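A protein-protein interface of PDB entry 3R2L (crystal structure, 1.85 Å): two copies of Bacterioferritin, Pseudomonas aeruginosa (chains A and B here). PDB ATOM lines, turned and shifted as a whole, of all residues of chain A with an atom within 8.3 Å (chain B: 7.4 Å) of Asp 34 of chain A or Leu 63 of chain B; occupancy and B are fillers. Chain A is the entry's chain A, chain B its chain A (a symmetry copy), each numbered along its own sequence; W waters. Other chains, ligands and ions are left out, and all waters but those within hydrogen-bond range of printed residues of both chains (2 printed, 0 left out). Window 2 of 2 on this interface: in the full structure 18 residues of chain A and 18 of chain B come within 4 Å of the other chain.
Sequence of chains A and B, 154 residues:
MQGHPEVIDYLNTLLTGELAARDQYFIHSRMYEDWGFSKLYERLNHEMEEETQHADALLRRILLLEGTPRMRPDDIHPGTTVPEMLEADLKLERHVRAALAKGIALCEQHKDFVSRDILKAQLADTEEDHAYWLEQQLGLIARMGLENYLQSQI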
ATOM      1  N   PHE A  26       6.658 -22.528   7.864  1.00  0.00           N
ATOM      2  CA  PHE A  26       6.649 -23.839   7.136  1.00  0.00           C
ATOM      3  C   PHE A  26       7.623 -23.730   5.949  1.00  0.00           C
ATOM      4  O   PHE A  26       8.628 -24.456   5.824  1.00  0.00           O
ATOM      5  CB  PHE A  26       5.225 -24.163   6.645  1.00  0.00           C
ATOM      6  CG  PHE A  26       4.949 -25.651   6.326  1.00  0.00           C
ATOM      7  CD1 PHE A  26       3.649 -26.044   6.012  1.00  0.00           C
ATOM      8  CD2 PHE A  26       5.962 -26.617   6.310  1.00  0.00           C
ATOM      9  CE1 PHE A  26       3.322 -27.366   5.712  1.00  0.00           C
ATOM     10  CE2 PHE A  26       5.669 -27.965   6.022  1.00  0.00           C
ATOM     11  CZ  PHE A  26       4.344 -28.353   5.720  1.00  0.00           C
ATOM     12  N   ILE A  27       7.357 -22.790   5.053  1.00  0.00           N
ATOM     13  CA  ILE A  27       8.232 -22.643   3.920  1.00  0.00           C
ATOM     14  C   ILE A  27       9.637 -22.181   4.290  1.00  0.00           C
ATOM     15  O   ILE A  27      10.610 -22.728   3.764  1.00  0.00           O
ATOM     16  CB  ILE A  27       7.604 -21.728   2.802  1.00  0.00           C
ATOM     17  CG1 ILE A  27       8.545 -21.630   1.601  1.00  0.00           C
ATOM     18  CG2 ILE A  27       7.288 -20.345   3.341  1.00  0.00           C
ATOM     19  CD1 ILE A  27       8.713 -22.933   0.863  1.00  0.00           C
ATOM     20  N   HIS A  28       9.810 -21.199   5.173  1.00  0.00           N
ATOM     21  CA  HIS A  28      11.197 -20.788   5.468  1.00  0.00           C
ATOM     22  C   HIS A  28      12.010 -21.920   6.097  1.00  0.00           C
ATOM     23  O   HIS A  28      13.214 -22.064   5.798  1.00  0.00           O
ATOM     24  CB  HIS A  28      11.266 -19.581   6.406  1.00  0.00           C
ATOM     25  CG  HIS A  28      10.955 -18.255   5.748  1.00  0.00           C
ATOM     26  ND1 HIS A  28      10.671 -17.122   6.486  1.00  0.00           N
ATOM     27  CD2 HIS A  28      10.953 -17.865   4.446  1.00  0.00           C
ATOM     28  CE1 HIS A  28      10.495 -16.092   5.670  1.00  0.00           C
ATOM     29  NE2 HIS A  28      10.657 -16.514   4.426  1.00  0.00           N
ATOM     30  N   SER A  29      11.412 -22.678   7.021  1.00  0.00           N
ATOM     31  CA  SER A  29      12.181 -23.746   7.668  1.00  0.00           C
ATOM     32  C   SER A  29      12.643 -24.770   6.639  1.00  0.00           C
ATOM     33  O   SER A  29      13.812 -25.207   6.668  1.00  0.00           O
ATOM     34  CB  SER A  29      11.407 -24.438   8.796  1.00  0.00           C
ATOM     35  OG  SER A  29      10.158 -24.972   8.344  1.00  0.00           O
ATOM     36  N   ARG A  30      11.764 -25.122   5.705  1.00  0.00           N
ATOM     37  CA  ARG A  30      12.152 -26.105   4.700  1.00  0.00           C
ATOM     38  C   ARG A  30      13.179 -25.532   3.721  1.00  0.00           C
ATOM     39  O   ARG A  30      14.030 -26.267   3.213  1.00  0.00           O
ATOM     40  CB  ARG A  30      10.926 -26.677   3.976  1.00  0.00           C
ATOM     41  CG  ARG A  30      10.304 -27.893   4.732  1.00  0.00           C
ATOM     42  CD  ARG A  30       9.813 -27.513   6.155  1.00  0.00           C
ATOM     43  NE  ARG A  30       9.165 -28.672   6.832  1.00  0.00           N
ATOM     44  CZ  ARG A  30       8.860 -28.708   8.127  1.00  0.00           C
ATOM     45  NH1 ARG A  30       9.127 -27.654   8.906  1.00  0.00           N
ATOM     46  NH2 ARG A  30       8.265 -29.783   8.651  1.00  0.00           N
ATOM     47  N   MET A  31      13.123 -24.231   3.455  1.00  0.00           N
ATOM     48  CA  MET A  31      14.121 -23.614   2.571  1.00  0.00           C
ATOM     49  C   MET A  31      15.483 -23.653   3.251  1.00  0.00           C
ATOM     50  O   MET A  31      16.511 -23.902   2.613  1.00  0.00           O
ATOM     51  CB  MET A  31      13.720 -22.164   2.260  1.00  0.00           C
ATOM     52  CG  MET A  31      12.584 -22.090   1.191  1.00  0.00           C
ATOM     53  SD  MET A  31      12.027 -20.359   1.074  1.00  0.00           S
ATOM     54  CE  MET A  31      13.486 -19.606   0.344  1.00  0.00           C
ATOM     55  N   TYR A  32      15.487 -23.376   4.552  1.00  0.00           N
ATOM     56  CA  TYR A  32      16.724 -23.398   5.326  1.00  0.00           C
ATOM     57  C   TYR A  32      17.316 -24.798   5.273  1.00  0.00           C
ATOM     58  O   TYR A  32      18.541 -24.956   5.124  1.00  0.00           O
ATOM     59  CB  TYR A  32      16.449 -23.041   6.790  1.00  0.00           C
ATOM     60  CG  TYR A  32      16.203 -21.578   7.047  1.00  0.00           C
ATOM     61  CD1 TYR A  32      17.009 -20.588   6.462  1.00  0.00           C
ATOM     62  CD2 TYR A  32      15.230 -21.181   7.924  1.00  0.00           C
ATOM     63  CE1 TYR A  32      16.797 -19.227   6.735  1.00  0.00           C
ATOM     64  CE2 TYR A  32      15.004 -19.818   8.209  1.00  0.00           C
ATOM     65  CZ  TYR A  32      15.789 -18.851   7.601  1.00  0.00           C
ATOM     66  OH  TYR A  32      15.567 -17.521   7.900  1.00  0.00           O
ATOM     67  N   GLU A  33      16.468 -25.822   5.417  1.00  0.00           N
ATOM     68  CA  GLU A  33      16.960 -27.204   5.400  1.00  0.00           C
ATOM     69  C   GLU A  33      17.487 -27.572   4.010  1.00  0.00           C
ATOM     70  O   GLU A  33      18.486 -28.277   3.892  1.00  0.00           O
ATOM     71  CB  GLU A  33      15.853 -28.182   5.832  1.00  0.00           C
ATOM     72  CG  GLU A  33      16.262 -29.640   5.786  1.00  0.00           C
ATOM     73  CD  GLU A  33      17.381 -30.003   6.782  1.00  0.00           C
ATOM     74  OE1 GLU A  33      17.948 -31.118   6.630  1.00  0.00           O
ATOM     75  OE2 GLU A  33      17.707 -29.191   7.686  1.00  0.00           O
ATOM     76  N   ASP A  34      16.789 -27.116   2.969  1.00  0.00           N
ATOM     77  CA  ASP A  34      17.174 -27.321   1.550  1.00  0.00           C
ATOM     78  C   ASP A  34      18.601 -26.796   1.317  1.00  0.00           C
ATOM     79  O   ASP A  34      19.390 -27.402   0.571  1.00  0.00           O
ATOM     80  CB  ASP A  34      16.155 -26.583   0.651  1.00  0.00           C
ATOM     81  CG  ASP A  34      16.545 -26.554  -0.856  1.00  0.00           C
ATOM     82  OD1 ASP A  34      16.735 -27.633  -1.439  1.00  0.00           O
ATOM     83  OD2 ASP A  34      16.598 -25.436  -1.448  1.00  0.00           O
ATOM     84  N   TRP A  35      18.962 -25.702   1.998  1.00  0.00           N
ATOM     85  CA  TRP A  35      20.288 -25.130   1.834  1.00  0.00           C
ATOM     86  C   TRP A  35      21.346 -25.733   2.778  1.00  0.00           C
ATOM     87  O   TRP A  35      22.525 -25.369   2.713  1.00  0.00           O
ATOM     88  CB  TRP A  35      20.226 -23.611   2.041  1.00  0.00           C
ATOM     89  CG  TRP A  35      19.476 -22.874   0.977  1.00  0.00           C
ATOM     90  CD1 TRP A  35      19.335 -23.230  -0.339  1.00  0.00           C
ATOM     91  CD2 TRP A  35      18.776 -21.634   1.133  1.00  0.00           C
ATOM     92  NE1 TRP A  35      18.575 -22.281  -1.009  1.00  0.00           N
ATOM     93  CE2 TRP A  35      18.216 -21.304  -0.122  1.00  0.00           C
ATOM     94  CE3 TRP A  35      18.550 -20.778   2.224  1.00  0.00           C
ATOM     95  CZ2 TRP A  35      17.463 -20.148  -0.321  1.00  0.00           C
ATOM     96  CZ3 TRP A  35      17.806 -19.644   2.031  1.00  0.00           C
ATOM     97  CH2 TRP A  35      17.265 -19.335   0.761  1.00  0.00           C
ATOM     98  N   GLY A  36      20.933 -26.614   3.680  1.00  0.00           N
ATOM     99  CA  GLY A  36      21.884 -27.193   4.632  1.00  0.00           C
ATOM    100  C   GLY A  36      22.053 -26.451   5.957  1.00  0.00           C
ATOM    101  O   GLY A  36      22.972 -26.757   6.700  1.00  0.00           O
ATOM    102  N   PHE A  37      21.174 -25.499   6.294  1.00  0.00           N
ATOM    103  CA  PHE A  37      21.264 -24.838   7.602  1.00  0.00           C
ATOM    104  C   PHE A  37      20.328 -25.499   8.597  1.00  0.00           C
ATOM    105  O   PHE A  37      19.204 -25.014   8.827  1.00  0.00           O
ATOM    106  CB  PHE A  37      20.927 -23.349   7.449  1.00  0.00           C
ATOM    107  CG  PHE A  37      21.876 -22.627   6.499  1.00  0.00           C
ATOM    108  CD1 PHE A  37      23.236 -22.601   6.762  1.00  0.00           C
ATOM    109  CD2 PHE A  37      21.408 -22.045   5.339  1.00  0.00           C
ATOM    110  CE1 PHE A  37      24.120 -21.986   5.859  1.00  0.00           C
ATOM    111  CE2 PHE A  37      22.282 -21.429   4.456  1.00  0.00           C
ATOM    112  CZ  PHE A  37      23.621 -21.403   4.724  1.00  0.00           C
ATOM    113  N   SER A  38      20.759 -26.625   9.172  1.00  0.00           N
ATOM    114  CA  SER A  38      19.824 -27.416   9.970  1.00  0.00           C
ATOM    115  C   SER A  38      19.433 -26.715  11.279  1.00  0.00           C
ATOM    116  O   SER A  38      18.339 -26.938  11.794  1.00  0.00           O
ATOM    117  CB  SER A  38      20.362 -28.836  10.201  1.00  0.00           C
ATOM    118  OG  SER A  38      20.251 -29.587   8.992  1.00  0.00           O
ATOM    119  N   TYR A  41      16.556 -24.585  10.311  1.00  0.00           N
ATOM    120  CA  TYR A  41      15.418 -25.472  10.082  1.00  0.00           C
ATOM    121  C   TYR A  41      14.777 -25.829  11.411  1.00  0.00           C
ATOM    122  O   TYR A  41      13.550 -25.772  11.559  1.00  0.00           O
ATOM    123  CB  TYR A  41      15.826 -26.777   9.364  1.00  0.00           C
ATOM    124  CG  TYR A  41      14.757 -27.828   9.508  1.00  0.00           C
ATOM    125  CD1 TYR A  41      14.855 -28.815  10.497  1.00  0.00           C
ATOM    126  CD2 TYR A  41      13.633 -27.826   8.691  1.00  0.00           C
ATOM    127  CE1 TYR A  41      13.842 -29.781  10.675  1.00  0.00           C
ATOM    128  CE2 TYR A  41      12.635 -28.805   8.834  1.00  0.00           C
ATOM    129  CZ  TYR A  41      12.750 -29.776   9.838  1.00  0.00           C
ATOM    130  OH  TYR A  41      11.742 -30.720   9.995  1.00  0.00           O
ATOM    131  N   MET B   1      19.037 -30.380  -8.580  1.00  0.00           N
ATOM    132  CA  MET B   1      18.654 -30.995  -9.900  1.00  0.00           C
ATOM    133  C   MET B   1      17.344 -30.317 -10.349  1.00  0.00           C
ATOM    134  O   MET B   1      16.409 -30.237  -9.575  1.00  0.00           O
ATOM    135  CB  MET B   1      18.451 -32.520  -9.717  1.00  0.00           C
ATOM    136  CG  MET B   1      17.953 -33.286 -10.960  1.00  0.00           C
ATOM    137  SD  MET B   1      17.384 -35.029 -10.693  1.00  0.00           S
ATOM    138  CE  MET B   1      16.071 -34.897  -9.445  1.00  0.00           C
ATOM    139  N   ILE B   8       6.816 -30.025 -11.596  1.00  0.00           N
ATOM    140  CA  ILE B   8       6.891 -29.061 -10.510  1.00  0.00           C
ATOM    141  C   ILE B   8       5.574 -28.339 -10.387  1.00  0.00           C
ATOM    142  O   ILE B   8       5.029 -28.229  -9.297  1.00  0.00           O
ATOM    143  CB  ILE B   8       8.088 -28.084 -10.687  1.00  0.00           C
ATOM    144  CG1 ILE B   8       9.426 -28.804 -10.481  1.00  0.00           C
ATOM    145  CG2 ILE B   8       7.955 -26.890  -9.758  1.00  0.00           C
ATOM    146  CD1 ILE B   8      10.639 -28.069 -11.049  1.00  0.00           C
ATOM    147  N   LEU B  11       3.018 -30.697  -8.859  1.00  0.00           N
ATOM    148  CA  LEU B  11       3.283 -30.932  -7.417  1.00  0.00           C
ATOM    149  C   LEU B  11       2.784 -29.744  -6.633  1.00  0.00           C
ATOM    150  O   LEU B  11       2.221 -29.896  -5.548  1.00  0.00           O
ATOM    151  CB  LEU B  11       4.782 -31.128  -7.156  1.00  0.00           C
ATOM    152  CG  LEU B  11       5.414 -32.365  -7.814  1.00  0.00           C
ATOM    153  CD1 LEU B  11       6.895 -32.397  -7.499  1.00  0.00           C
ATOM    154  CD2 LEU B  11       4.736 -33.654  -7.333  1.00  0.00           C
ATOM    155  N   ALA B  57       6.051 -33.431   2.519  1.00  0.00           N
ATOM    156  CA  ALA B  57       6.776 -34.251   1.524  1.00  0.00           C
ATOM    157  C   ALA B  57       6.758 -33.557   0.134  1.00  0.00           C
ATOM    158  O   ALA B  57       7.769 -33.543  -0.583  1.00  0.00           O
ATOM    159  CB  ALA B  57       6.161 -35.643   1.445  1.00  0.00           C
ATOM    160  N   LEU B  58       5.613 -32.978  -0.233  1.00  0.00           N
ATOM    161  CA  LEU B  58       5.502 -32.294  -1.536  1.00  0.00           C
ATOM    162  C   LEU B  58       6.351 -31.052  -1.571  1.00  0.00           C
ATOM    163  O   LEU B  58       7.090 -30.818  -2.533  1.00  0.00           O
ATOM    164  CB  LEU B  58       4.037 -31.927  -1.820  1.00  0.00           C
ATOM    165  CG  LEU B  58       3.081 -33.104  -1.991  1.00  0.00           C
ATOM    166  CD1 LEU B  58       1.609 -32.633  -2.074  1.00  0.00           C
ATOM    167  CD2 LEU B  58       3.379 -33.945  -3.234  1.00  0.00           C
ATOM    168  N   LEU B  59       6.242 -30.241  -0.529  1.00  0.00           N
ATOM    169  CA  LEU B  59       7.042 -29.034  -0.431  1.00  0.00           C
ATOM    170  C   LEU B  59       8.540 -29.336  -0.573  1.00  0.00           C
ATOM    171  O   LEU B  59       9.278 -28.672  -1.314  1.00  0.00           O
ATOM    172  CB  LEU B  59       6.768 -28.399   0.928  1.00  0.00           C
ATOM    173  CG  LEU B  59       7.230 -26.961   1.189  1.00  0.00           C
ATOM    174  CD1 LEU B  59       6.502 -26.472   2.489  1.00  0.00           C
ATOM    175  CD2 LEU B  59       8.678 -26.898   1.361  1.00  0.00           C
ATOM    176  N   ARG B  60       9.034 -30.298   0.197  1.00  0.00           N
ATOM    177  CA  ARG B  60      10.467 -30.614   0.140  1.00  0.00           C
ATOM    178  C   ARG B  60      10.897 -31.116  -1.232  1.00  0.00           C
ATOM    179  O   ARG B  60      12.007 -30.823  -1.685  1.00  0.00           O
ATOM    180  CB  ARG B  60      10.824 -31.689   1.171  1.00  0.00           C
ATOM    181  CG  ARG B  60      10.701 -31.123   2.614  1.00  0.00           C
ATOM    182  CD  ARG B  60      11.230 -32.115   3.644  1.00  0.00           C
ATOM    183  NE  ARG B  60      10.711 -31.832   4.976  1.00  0.00           N
ATOM    184  CZ  ARG B  60      11.425 -31.797   6.106  1.00  0.00           C
ATOM    185  NH1 ARG B  60      12.724 -31.997   6.089  1.00  0.00           N
ATOM    186  NH2 ARG B  60      10.819 -31.593   7.272  1.00  0.00           N
ATOM    187  N   ARG B  61      10.044 -31.904  -1.867  1.00  0.00           N
ATOM    188  CA  ARG B  61      10.368 -32.471  -3.181  1.00  0.00           C
ATOM    189  C   ARG B  61      10.449 -31.323  -4.216  1.00  0.00           C
ATOM    190  O   ARG B  61      11.360 -31.274  -5.029  1.00  0.00           O
ATOM    191  CB  ARG B  61       9.271 -33.434  -3.605  1.00  0.00           C
ATOM    192  CG  ARG B  61       9.512 -34.045  -4.965  1.00  0.00           C
ATOM    193  CD  ARG B  61      10.829 -34.858  -5.001  1.00  0.00           C
ATOM    194  NE  ARG B  61      10.983 -35.490  -6.309  1.00  0.00           N
ATOM    195  CZ  ARG B  61      12.089 -36.118  -6.707  1.00  0.00           C
ATOM    196  NH1 ARG B  61      13.143 -36.250  -5.876  1.00  0.00           N
ATOM    197  NH2 ARG B  61      12.144 -36.606  -7.942  1.00  0.00           N
ATOM    198  N   ILE B  62       9.505 -30.393  -4.140  1.00  0.00           N
ATOM    199  CA  ILE B  62       9.508 -29.198  -5.015  1.00  0.00           C
ATOM    200  C   ILE B  62      10.789 -28.399  -4.829  1.00  0.00           C
ATOM    201  O   ILE B  62      11.426 -28.000  -5.809  1.00  0.00           O
ATOM    202  CB  ILE B  62       8.282 -28.304  -4.731  1.00  0.00           C
ATOM    203  CG1 ILE B  62       6.999 -28.945  -5.283  1.00  0.00           C
ATOM    204  CG2 ILE B  62       8.464 -26.925  -5.361  1.00  0.00           C
ATOM    205  CD1 ILE B  62       5.678 -28.536  -4.533  1.00  0.00           C
ATOM    206  N   LEU B  63      11.216 -28.179  -3.582  1.00  0.00           N
ATOM    207  CA  LEU B  63      12.490 -27.479  -3.346  1.00  0.00           C
ATOM    208  C   LEU B  63      13.685 -28.268  -3.899  1.00  0.00           C
ATOM    209  O   LEU B  63      14.614 -27.698  -4.504  1.00  0.00           O
ATOM    210  CB  LEU B  63      12.682 -27.198  -1.845  1.00  0.00           C
ATOM    211  CG  LEU B  63      11.800 -26.120  -1.205  1.00  0.00           C
ATOM    212  CD1 LEU B  63      12.050 -26.155   0.337  1.00  0.00           C
ATOM    213  CD2 LEU B  63      12.088 -24.649  -1.816  1.00  0.00           C
ATOM    214  N   LEU B  64      13.687 -29.594  -3.710  1.00  0.00           N
ATOM    215  CA  LEU B  64      14.809 -30.391  -4.206  1.00  0.00           C
ATOM    216  C   LEU B  64      14.926 -30.243  -5.732  1.00  0.00           C
ATOM    217  O   LEU B  64      16.013 -30.260  -6.297  1.00  0.00           O
ATOM    218  CB  LEU B  64      14.616 -31.855  -3.854  1.00  0.00           C
ATOM    219  CG  LEU B  64      15.640 -32.879  -4.376  1.00  0.00           C
ATOM    220  CD1 LEU B  64      15.500 -34.170  -3.562  1.00  0.00           C
ATOM    221  CD2 LEU B  64      15.381 -33.147  -5.812  1.00  0.00           C
ATOM    222  N   LEU B  65      13.776 -30.144  -6.381  1.00  0.00           N
ATOM    223  CA  LEU B  65      13.695 -30.054  -7.838  1.00  0.00           C
ATOM    224  C   LEU B  65      13.888 -28.585  -8.295  1.00  0.00           C
ATOM    225  O   LEU B  65      13.688 -28.249  -9.477  1.00  0.00           O
ATOM    226  CB  LEU B  65      12.338 -30.559  -8.323  1.00  0.00           C
ATOM    227  CG  LEU B  65      12.038 -32.061  -8.125  1.00  0.00           C
ATOM    228  CD1 LEU B  65      10.634 -32.425  -8.623  1.00  0.00           C
ATOM    229  CD2 LEU B  65      13.109 -32.885  -8.784  1.00  0.00           C
ATOM    230  N   GLU B  66      14.249 -27.723  -7.353  1.00  0.00           N
ATOM    231  CA  GLU B  66      14.572 -26.319  -7.631  1.00  0.00           C
ATOM    232  C   GLU B  66      13.372 -25.480  -8.044  1.00  0.00           C
ATOM    233  O   GLU B  66      13.511 -24.443  -8.706  1.00  0.00           O
ATOM    234  CB  GLU B  66      15.717 -26.239  -8.669  1.00  0.00           C
ATOM    235  CG  GLU B  66      16.945 -27.033  -8.161  1.00  0.00           C
ATOM    236  CD  GLU B  66      18.189 -26.882  -8.998  1.00  0.00           C
ATOM    237  OE1 GLU B  66      18.316 -25.835  -9.656  1.00  0.00           O
ATOM    238  OE2 GLU B  66      19.034 -27.814  -8.997  1.00  0.00           O
ATOM    239  N   GLY B  67      12.190 -25.922  -7.645  1.00  0.00           N
ATOM    240  CA  GLY B  67      10.980 -25.120  -7.822  1.00  0.00           C
ATOM    241  C   GLY B  67      10.703 -24.227  -6.639  1.00  0.00           C
ATOM    242  O   GLY B  67      11.416 -24.266  -5.625  1.00  0.00           O
ATOM    243  N   THR B  68       9.646 -23.438  -6.738  1.00  0.00           N
ATOM    244  CA  THR B  68       9.255 -22.513  -5.681  1.00  0.00           C
ATOM    245  C   THR B  68       7.891 -22.981  -5.173  1.00  0.00           C
ATOM    246  O   THR B  68       6.929 -23.006  -5.936  1.00  0.00           O
ATOM    247  CB  THR B  68       9.167 -21.060  -6.241  1.00  0.00           C
ATOM    248  OG1 THR B  68      10.447 -20.674  -6.754  1.00  0.00           O
ATOM    249  CG2 THR B  68       8.716 -20.062  -5.162  1.00  0.00           C
ATOM    250  N   PRO B  69       7.799 -23.399  -3.888  1.00  0.00           N
ATOM    251  CA  PRO B  69       6.490 -23.929  -3.505  1.00  0.00           C
ATOM    252  C   PRO B  69       5.415 -22.839  -3.413  1.00  0.00           C
ATOM    253  O   PRO B  69       5.699 -21.704  -3.050  1.00  0.00           O
ATOM    254  CB  PRO B  69       6.751 -24.601  -2.130  1.00  0.00           C
ATOM    255  CG  PRO B  69       8.248 -24.932  -2.151  1.00  0.00           C
ATOM    256  CD  PRO B  69       8.851 -23.722  -2.896  1.00  0.00           C
HETATM  257  O   HOH W   1      17.389 -27.525  -4.374  1.00  0.00           O
HETATM  258  O   HOH W   2      15.615 -25.274  -4.013  1.00  0.00           O
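NH2 of Arg 60 of chain B is in hydrogen-bond range of OH of Tyr 41 of chain A (3.0 Å).
The guanidinium group of Arg 30 of chain A lies close to the guanidinium group of Arg 60 of chain B (3.4 Å).
OG of Ser 29 of chain A lies within hydrogen-bond range of O of Phe 26 of chain A, 3.0 Å away.
The guanidinium group (NH1) of Arg 30 of chain A is in hydrogen-bond range of the side-chain hydroxyl (OG) of Ser 29 of chain A (2.9 Å).
Among the printed residues, merely in contact across the chains: Phe 26 of chain A with Leu 59 of chain B (3.9 Å), Ile 27 of chain A with Leu 59 of chain B (3.996 Å), Ile 27 of chain A with Pro 69 of chain B (3.6 Å), Arg 30 of chain A with Leu 59 of chain B (3.5 Å), Arg 30 of chain A with Leu 63 of chain B (3.5 Å), Met 31 of chain A with Leu 63 of chain B (3.8 Å) and Asp 34 of chain A with Leu 63 of chain B (3.7 Å).
Of the printed residues of chain A, Pro 69 of chain B touches Ile 27 (3.6 Å).
Of the printed residues of chain B, Ile 27 of chain A touches Leu 59 (3.996 Å) and Pro 69 (3.6 Å).
Tyr 32 of chain A touches none of the printed residues of chain B.
Ile 8 of chain B touches none of the printed residues of chain A.
The nearest residue of chain B that does not touch Asp 34 of chain A is Leu 64 of chain B (4.3 Å).
Of the 16 printed residues of chain B, 4 touch a printed residue of chain A.
Printed residues of chain A that touch a printed residue of chain B: Phe 26, Ile 27, Arg 30, Met 31, Asp 34 and Tyr 41.
Hydrophobic or aromatic side chains of chain A within 4 Å of the printed part of chain B: Phe 26, Ile 27, Met 31 and Tyr 41.
No position is printed for both chains.
Of the 9 pairs that touch across the chains among the printed residues, none has its exchanged pair printed and touching as well.
Water W2 bridges the backbone carbonyl oxygen of Leu 63 of chain B (2.7 Å) and the side-chain carboxylate of Asp 34 of chain A (2.8 Å).
Water W1 lies within hydrogen-bond range of O of Leu 63 of chain B (2.8 Å) and OD1 of Asp 34 of chain A (3.0 Å).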
